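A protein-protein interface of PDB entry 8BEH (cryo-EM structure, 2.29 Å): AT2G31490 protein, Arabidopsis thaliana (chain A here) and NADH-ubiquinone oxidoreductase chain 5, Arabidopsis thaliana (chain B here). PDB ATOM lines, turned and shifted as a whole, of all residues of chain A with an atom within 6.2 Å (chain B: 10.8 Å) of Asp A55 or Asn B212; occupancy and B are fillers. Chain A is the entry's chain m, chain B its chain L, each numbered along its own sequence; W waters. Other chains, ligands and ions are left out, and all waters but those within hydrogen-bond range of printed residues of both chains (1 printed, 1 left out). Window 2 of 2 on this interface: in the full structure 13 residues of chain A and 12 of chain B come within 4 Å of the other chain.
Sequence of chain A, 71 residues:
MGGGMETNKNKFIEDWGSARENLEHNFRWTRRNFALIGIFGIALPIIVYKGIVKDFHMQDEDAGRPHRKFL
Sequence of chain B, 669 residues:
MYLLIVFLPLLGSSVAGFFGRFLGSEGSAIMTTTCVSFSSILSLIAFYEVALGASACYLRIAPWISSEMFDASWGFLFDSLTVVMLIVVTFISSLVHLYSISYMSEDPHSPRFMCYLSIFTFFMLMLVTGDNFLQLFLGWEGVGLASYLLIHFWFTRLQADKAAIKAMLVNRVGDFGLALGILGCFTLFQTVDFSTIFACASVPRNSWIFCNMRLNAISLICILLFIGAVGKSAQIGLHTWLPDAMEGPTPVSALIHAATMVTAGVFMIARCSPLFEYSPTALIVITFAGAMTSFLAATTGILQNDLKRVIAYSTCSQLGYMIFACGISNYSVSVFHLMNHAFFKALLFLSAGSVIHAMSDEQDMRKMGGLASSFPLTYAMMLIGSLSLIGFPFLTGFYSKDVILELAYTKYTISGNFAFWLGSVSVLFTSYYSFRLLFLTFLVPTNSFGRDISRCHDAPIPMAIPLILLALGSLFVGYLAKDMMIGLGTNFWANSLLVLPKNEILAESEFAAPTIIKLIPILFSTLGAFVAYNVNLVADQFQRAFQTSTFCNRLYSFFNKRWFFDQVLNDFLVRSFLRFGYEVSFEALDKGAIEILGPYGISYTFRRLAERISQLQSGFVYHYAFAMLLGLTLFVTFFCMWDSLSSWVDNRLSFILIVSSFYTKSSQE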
ATOM      1  N   LYS A  50      29.582   3.766  -9.975  1.00  0.00           N
ATOM      2  CA  LYS A  50      28.083   3.728 -10.089  1.00  0.00           C
ATOM      3  C   LYS A  50      27.448   4.152  -8.747  1.00  0.00           C
ATOM      4  O   LYS A  50      26.582   4.978  -8.808  1.00  0.00           O
ATOM      5  CB  LYS A  50      27.625   2.420 -10.748  1.00  0.00           C
ATOM      6  CG  LYS A  50      27.937   2.334 -12.228  1.00  0.00           C
ATOM      7  CD  LYS A  50      27.293   1.155 -12.895  1.00  0.00           C
ATOM      8  CE  LYS A  50      27.576   1.140 -14.378  1.00  0.00           C
ATOM      9  NZ  LYS A  50      27.138   2.398 -15.024  1.00  0.00           N
ATOM     10  N   GLY A  51      28.039   3.793  -7.614  1.00  0.00           N
ATOM     11  CA  GLY A  51      27.578   4.226  -6.285  1.00  0.00           C
ATOM     12  C   GLY A  51      27.672   5.719  -6.075  1.00  0.00           C
ATOM     13  O   GLY A  51      26.679   6.279  -5.708  1.00  0.00           O
ATOM     14  N   ILE A  52      28.806   6.321  -6.422  1.00  0.00           N
ATOM     15  CA  ILE A  52      29.089   7.752  -6.256  1.00  0.00           C
ATOM     16  C   ILE A  52      28.123   8.526  -7.136  1.00  0.00           C
ATOM     17  O   ILE A  52      27.584   9.490  -6.625  1.00  0.00           O
ATOM     18  CB  ILE A  52      30.621   8.046  -6.460  1.00  0.00           C
ATOM     19  CG1 ILE A  52      31.490   7.378  -5.393  1.00  0.00           C
ATOM     20  CG2 ILE A  52      30.901   9.536  -6.595  1.00  0.00           C
ATOM     21  CD1 ILE A  52      32.963   7.390  -5.678  1.00  0.00           C
ATOM     22  N   VAL A  53      27.896   8.072  -8.361  1.00  0.00           N
ATOM     23  CA  VAL A  53      27.047   8.782  -9.341  1.00  0.00           C
ATOM     24  C   VAL A  53      25.587   8.756  -8.873  1.00  0.00           C
ATOM     25  O   VAL A  53      24.975   9.759  -8.906  1.00  0.00           O
ATOM     26  CB  VAL A  53      27.257   8.307 -10.808  1.00  0.00           C
ATOM     27  CG1 VAL A  53      26.148   8.735 -11.753  1.00  0.00           C
ATOM     28  CG2 VAL A  53      28.628   8.659 -11.359  1.00  0.00           C
ATOM     29  N   LYS A  54      25.147   7.613  -8.428  1.00  0.00           N
ATOM     30  CA  LYS A  54      23.784   7.412  -7.931  1.00  0.00           C
ATOM     31  C   LYS A  54      23.564   8.332  -6.719  1.00  0.00           C
ATOM     32  O   LYS A  54      22.519   8.901  -6.643  1.00  0.00           O
ATOM     33  CB  LYS A  54      23.578   5.927  -7.673  1.00  0.00           C
ATOM     34  CG  LYS A  54      22.459   5.586  -6.702  1.00  0.00           C
ATOM     35  CD  LYS A  54      22.063   4.135  -6.771  1.00  0.00           C
ATOM     36  CE  LYS A  54      20.670   3.870  -6.242  1.00  0.00           C
ATOM     37  NZ  LYS A  54      20.617   3.893  -4.762  1.00  0.00           N
ATOM     38  N   ASP A  55      24.537   8.406  -5.855  1.00  0.00           N
ATOM     39  CA  ASP A  55      24.477   9.298  -4.686  1.00  0.00           C
ATOM     40  C   ASP A  55      24.170  10.719  -5.176  1.00  0.00           C
ATOM     41  O   ASP A  55      23.126  11.226  -4.743  1.00  0.00           O
ATOM     42  CB  ASP A  55      25.751   9.123  -3.876  1.00  0.00           C
ATOM     43  CG  ASP A  55      25.830   9.959  -2.625  1.00  0.00           C
ATOM     44  OD1 ASP A  55      25.017   9.729  -1.722  1.00  0.00           O
ATOM     45  OD2 ASP A  55      26.691  10.841  -2.572  1.00  0.00           O
ATOM     46  N   PHE A  56      24.932  11.244  -6.142  1.00  0.00           N
ATOM     47  CA  PHE A  56      24.616  12.564  -6.712  1.00  0.00           C
ATOM     48  C   PHE A  56      23.186  12.608  -7.332  1.00  0.00           C
ATOM     49  O   PHE A  56      22.586  13.652  -7.228  1.00  0.00           O
ATOM     50  CB  PHE A  56      25.667  13.064  -7.713  1.00  0.00           C
ATOM     51  CG  PHE A  56      27.034  13.435  -7.184  1.00  0.00           C
ATOM     52  CD1 PHE A  56      27.209  14.514  -6.330  1.00  0.00           C
ATOM     53  CD2 PHE A  56      28.164  12.756  -7.606  1.00  0.00           C
ATOM     54  CE1 PHE A  56      28.468  14.884  -5.891  1.00  0.00           C
ATOM     55  CE2 PHE A  56      29.427  13.118  -7.161  1.00  0.00           C
ATOM     56  CZ  PHE A  56      29.582  14.188  -6.310  1.00  0.00           C
ATOM     57  N   HIS A  57      22.742  11.568  -8.021  1.00  0.00           N
ATOM     58  CA  HIS A  57      21.418  11.538  -8.714  1.00  0.00           C
ATOM     59  C   HIS A  57      20.309  11.504  -7.681  1.00  0.00           C
ATOM     60  O   HIS A  57      19.305  12.136  -7.901  1.00  0.00           O
ATOM     61  CB  HIS A  57      21.353  10.344  -9.695  1.00  0.00           C
ATOM     62  CG  HIS A  57      22.156  10.501 -10.938  1.00  0.00           C
ATOM     63  ND1 HIS A  57      22.389   9.450 -11.808  1.00  0.00           N
ATOM     64  CD2 HIS A  57      22.749  11.579 -11.481  1.00  0.00           C
ATOM     65  CE1 HIS A  57      23.092   9.885 -12.822  1.00  0.00           C
ATOM     66  NE2 HIS A  57      23.329  11.177 -12.644  1.00  0.00           N
ATOM     67  N   MET A  58      20.547  10.782  -6.607  1.00  0.00           N
ATOM     68  CA  MET A  58      19.571  10.722  -5.518  1.00  0.00           C
ATOM     69  C   MET A  58      19.536  12.116  -4.879  1.00  0.00           C
ATOM     70  O   MET A  58      18.431  12.544  -4.589  1.00  0.00           O
ATOM     71  CB  MET A  58      19.811   9.542  -4.567  1.00  0.00           C
ATOM     72  CG  MET A  58      19.462   8.194  -5.114  1.00  0.00           C
ATOM     73  SD  MET A  58      20.018   6.879  -3.998  1.00  0.00           S
ATOM     74  CE  MET A  58      18.832   6.996  -2.661  1.00  0.00           C
ATOM     75  N   GLN A  59      20.655  12.801  -4.710  1.00  0.00           N
ATOM     76  CA  GLN A  59      20.611  14.194  -4.276  1.00  0.00           C
ATOM     77  C   GLN A  59      19.868  15.057  -5.288  1.00  0.00           C
ATOM     78  O   GLN A  59      19.112  15.958  -4.912  1.00  0.00           O
ATOM     79  CB  GLN A  59      22.020  14.736  -4.061  1.00  0.00           C
ATOM     80  CG  GLN A  59      22.657  14.371  -2.735  1.00  0.00           C
ATOM     81  CD  GLN A  59      24.083  14.884  -2.630  1.00  0.00           C
ATOM     82  OE1 GLN A  59      24.344  15.893  -1.980  1.00  0.00           O
ATOM     83  NE2 GLN A  59      25.008  14.199  -3.286  1.00  0.00           N
ATOM     84  N   ASP A  60      20.082  14.800  -6.580  1.00  0.00           N
ATOM     85  CA  ASP A  60      19.441  15.601  -7.619  1.00  0.00           C
ATOM     86  C   ASP A  60      17.924  15.486  -7.545  1.00  0.00           C
ATOM     87  O   ASP A  60      17.209  16.493  -7.577  1.00  0.00           O
ATOM     88  CB  ASP A  60      19.938  15.168  -8.996  1.00  0.00           C
ATOM     89  CG  ASP A  60      21.208  15.874  -9.399  1.00  0.00           C
ATOM     90  OD1 ASP A  60      21.517  16.916  -8.791  1.00  0.00           O
ATOM     91  OD2 ASP A  60      21.900  15.385 -10.317  1.00  0.00           O
ATOM     92  N   SER B 207      15.369  14.230   5.259  1.00  0.00           N
ATOM     93  CA  SER B 207      15.945  12.941   4.924  1.00  0.00           C
ATOM     94  C   SER B 207      17.279  13.144   4.222  1.00  0.00           C
ATOM     95  O   SER B 207      17.529  14.184   3.611  1.00  0.00           O
ATOM     96  CB  SER B 207      14.999  12.136   4.035  1.00  0.00           C
ATOM     97  OG  SER B 207      15.269  10.750   4.125  1.00  0.00           O
ATOM     98  N   TRP B 208      18.134  12.135   4.307  1.00  0.00           N
ATOM     99  CA  TRP B 208      19.478  12.229   3.772  1.00  0.00           C
ATOM    100  C   TRP B 208      19.766  11.027   2.891  1.00  0.00           C
ATOM    101  O   TRP B 208      19.165   9.961   3.036  1.00  0.00           O
ATOM    102  CB  TRP B 208      20.512  12.316   4.890  1.00  0.00           C
ATOM    103  CG  TRP B 208      20.866  13.705   5.249  1.00  0.00           C
ATOM    104  CD1 TRP B 208      20.318  14.844   4.745  1.00  0.00           C
ATOM    105  CD2 TRP B 208      21.825  14.117   6.221  1.00  0.00           C
ATOM    106  NE1 TRP B 208      20.889  15.943   5.332  1.00  0.00           N
ATOM    107  CE2 TRP B 208      21.817  15.522   6.246  1.00  0.00           C
ATOM    108  CE3 TRP B 208      22.695  13.433   7.071  1.00  0.00           C
ATOM    109  CZ2 TRP B 208      22.645  16.258   7.088  1.00  0.00           C
ATOM    110  CZ3 TRP B 208      23.516  14.164   7.903  1.00  0.00           C
ATOM    111  CH2 TRP B 208      23.485  15.560   7.906  1.00  0.00           C
ATOM    112  N   ILE B 209      20.701  11.216   1.972  1.00  0.00           N
ATOM    113  CA  ILE B 209      21.198  10.143   1.127  1.00  0.00           C
ATOM    114  C   ILE B 209      22.493   9.648   1.754  1.00  0.00           C
ATOM    115  O   ILE B 209      23.515  10.341   1.726  1.00  0.00           O
ATOM    116  CB  ILE B 209      21.412  10.613  -0.316  1.00  0.00           C
ATOM    117  CG1 ILE B 209      20.102  11.165  -0.885  1.00  0.00           C
ATOM    118  CG2 ILE B 209      21.963   9.479  -1.164  1.00  0.00           C
ATOM    119  CD1 ILE B 209      19.015  10.129  -1.055  1.00  0.00           C
ATOM    120  N   PHE B 210      22.450   8.457   2.340  1.00  0.00           N
ATOM    121  CA  PHE B 210      23.624   7.842   2.945  1.00  0.00           C
ATOM    122  C   PHE B 210      23.831   6.475   2.314  1.00  0.00           C
ATOM    123  O   PHE B 210      23.004   5.574   2.493  1.00  0.00           O
ATOM    124  CB  PHE B 210      23.483   7.720   4.460  1.00  0.00           C
ATOM    125  CG  PHE B 210      24.760   7.356   5.142  1.00  0.00           C
ATOM    126  CD1 PHE B 210      25.782   8.282   5.263  1.00  0.00           C
ATOM    127  CD2 PHE B 210      24.960   6.076   5.623  1.00  0.00           C
ATOM    128  CE1 PHE B 210      26.969   7.945   5.879  1.00  0.00           C
ATOM    129  CE2 PHE B 210      26.144   5.734   6.240  1.00  0.00           C
ATOM    130  CZ  PHE B 210      27.152   6.669   6.366  1.00  0.00           C
ATOM    131  N   CYS B 211      24.944   6.324   1.603  1.00  0.00           N
ATOM    132  CA  CYS B 211      25.270   5.094   0.888  1.00  0.00           C
ATOM    133  C   CYS B 211      24.092   4.624   0.040  1.00  0.00           C
ATOM    134  O   CYS B 211      23.617   3.492   0.153  1.00  0.00           O
ATOM    135  CB  CYS B 211      25.738   4.008   1.853  1.00  0.00           C
ATOM    136  SG  CYS B 211      26.829   4.631   3.146  1.00  0.00           S
ATOM    137  N   ASN B 212      23.539   5.513  -0.767  1.00  0.00           N
ATOM    138  CA  ASN B 212      22.535   5.181  -1.801  1.00  0.00           C
ATOM    139  C   ASN B 212      21.224   4.775  -1.139  1.00  0.00           C
ATOM    140  O   ASN B 212      20.468   4.074  -1.739  1.00  0.00           O
ATOM    141  CB  ASN B 212      23.119   4.250  -2.878  1.00  0.00           C
ATOM    142  CG  ASN B 212      24.443   4.659  -3.489  1.00  0.00           C
ATOM    143  OD1 ASN B 212      25.119   3.829  -4.073  1.00  0.00           O
ATOM    144  ND2 ASN B 212      24.837   5.906  -3.358  1.00  0.00           N
ATOM    145  N   MET B 213      21.040   5.246   0.080  1.00  0.00           N
ATOM    146  CA  MET B 213      19.805   4.987   0.802  1.00  0.00           C
ATOM    147  C   MET B 213      19.253   6.302   1.336  1.00  0.00           C
ATOM    148  O   MET B 213      20.005   7.218   1.674  1.00  0.00           O
ATOM    149  CB  MET B 213      20.015   4.008   1.961  1.00  0.00           C
ATOM    150  CG  MET B 213      20.585   2.664   1.555  1.00  0.00           C
ATOM    151  SD  MET B 213      21.049   1.647   2.966  1.00  0.00           S
ATOM    152  CE  MET B 213      21.756   2.862   4.068  1.00  0.00           C
ATOM    153  N   ARG B 214      17.932   6.386   1.405  1.00  0.00           N
ATOM    154  CA  ARG B 214      17.248   7.557   1.938  1.00  0.00           C
ATOM    155  C   ARG B 214      16.898   7.277   3.394  1.00  0.00           C
ATOM    156  O   ARG B 214      16.111   6.372   3.681  1.00  0.00           O
ATOM    157  CB  ARG B 214      15.995   7.869   1.123  1.00  0.00           C
ATOM    158  CG  ARG B 214      15.860   9.320   0.714  1.00  0.00           C
ATOM    159  CD  ARG B 214      14.892   9.479  -0.444  1.00  0.00           C
ATOM    160  NE  ARG B 214      15.216   8.604  -1.563  1.00  0.00           N
ATOM    161  CZ  ARG B 214      15.700   9.016  -2.727  1.00  0.00           C
ATOM    162  NH1 ARG B 214      15.948  10.291  -2.960  1.00  0.00           N
ATOM    163  NH2 ARG B 214      15.941   8.123  -3.682  1.00  0.00           N
ATOM    164  N   LEU B 215      17.494   8.041   4.306  1.00  0.00           N
ATOM    165  CA  LEU B 215      17.332   7.827   5.738  1.00  0.00           C
ATOM    166  C   LEU B 215      17.046   9.150   6.437  1.00  0.00           C
ATOM    167  O   LEU B 215      17.314  10.228   5.905  1.00  0.00           O
ATOM    168  CB  LEU B 215      18.580   7.176   6.364  1.00  0.00           C
ATOM    169  CG  LEU B 215      19.474   6.230   5.556  1.00  0.00           C
ATOM    170  CD1 LEU B 215      20.671   5.792   6.381  1.00  0.00           C
ATOM    171  CD2 LEU B 215      18.701   5.010   5.097  1.00  0.00           C
ATOM    172  N   LEU B 220      20.347   8.800  11.483  1.00  0.00           N
ATOM    173  CA  LEU B 220      21.647   8.408  10.952  1.00  0.00           C
ATOM    174  C   LEU B 220      22.769   8.929  11.836  1.00  0.00           C
ATOM    175  O   LEU B 220      23.696   8.188  12.191  1.00  0.00           O
ATOM    176  CB  LEU B 220      21.795   8.931   9.522  1.00  0.00           C
ATOM    177  CG  LEU B 220      23.192   8.906   8.895  1.00  0.00           C
ATOM    178  CD1 LEU B 220      23.671   7.480   8.732  1.00  0.00           C
ATOM    179  CD2 LEU B 220      23.189   9.630   7.561  1.00  0.00           C
HETATM  180  O   HOH W   1      24.851  11.673  -0.253  1.00  0.00           O
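Among the printed residues, merely in contact across the chains: Asp A55 with Ile B209, Met A58 with Arg B214, Asp A55 with Asn B212, Met A58 with Ile B209 and Met A58 with Met B213.
Asp A55 touches just these residues of chain B: Ile B209 (3.1 Å) and Asn B212 (3.4 Å). Asn B212 touches just these residues of chain A: Gly A51, Lys A54, Asp A55 and Met A58. Of the printed residues of chain B, Lys A54 touches Asn B212 (3.0 Å). No residue of chain B comes within 4 Å of Phe A56. Of chain B, only Ile B209 (3.5 Å), Asn B212 (3.5 Å), Met B213 (3.9 Å) and Arg B214 (3.3 Å) come within 4 Å of Met A58. Gln A59 touches none of the printed residues of chain B. Of the printed residues of chain A, Met B213 touches Met A58. Printed residues of chain A within 4 Å of Arg B214: Met A58 (3.3 Å). Of the printed residues of chain A, Ile B209 touches Asp A55 and Met A58. Leu B215 touches none of the printed residues of chain A.
The side-chain amino group (NZ) of Lys A54 is in hydrogen-bond range of the side-chain sulfur (SD) of Met A58, 3.1 Å away.
ND2 of Asn B212 is in hydrogen-bond range of O of Gly A51, 3.0 Å away. The side-chain amino group (NZ) of Lys A54 sits at hydrogen-bond distance from the backbone carbonyl oxygen (O) of Asn B212 (3.0 Å). SD of Met A58 sits close to O of Asn B212.
Printed residues of chain B that touch a printed residue of chain A: Ile B209, Asn B212, Met B213 and Arg B214. Of the 11 printed residues of chain A, 4 touch a printed residue of chain B. Hydrophobic or aromatic side chains of chain A that line the printed part of chain B: Met A58. Among the printed residues, 8 pairs touch across the chains.
Water W1 lies within hydrogen-bond range of OD1 of Asp A55 and O of Ile B209.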
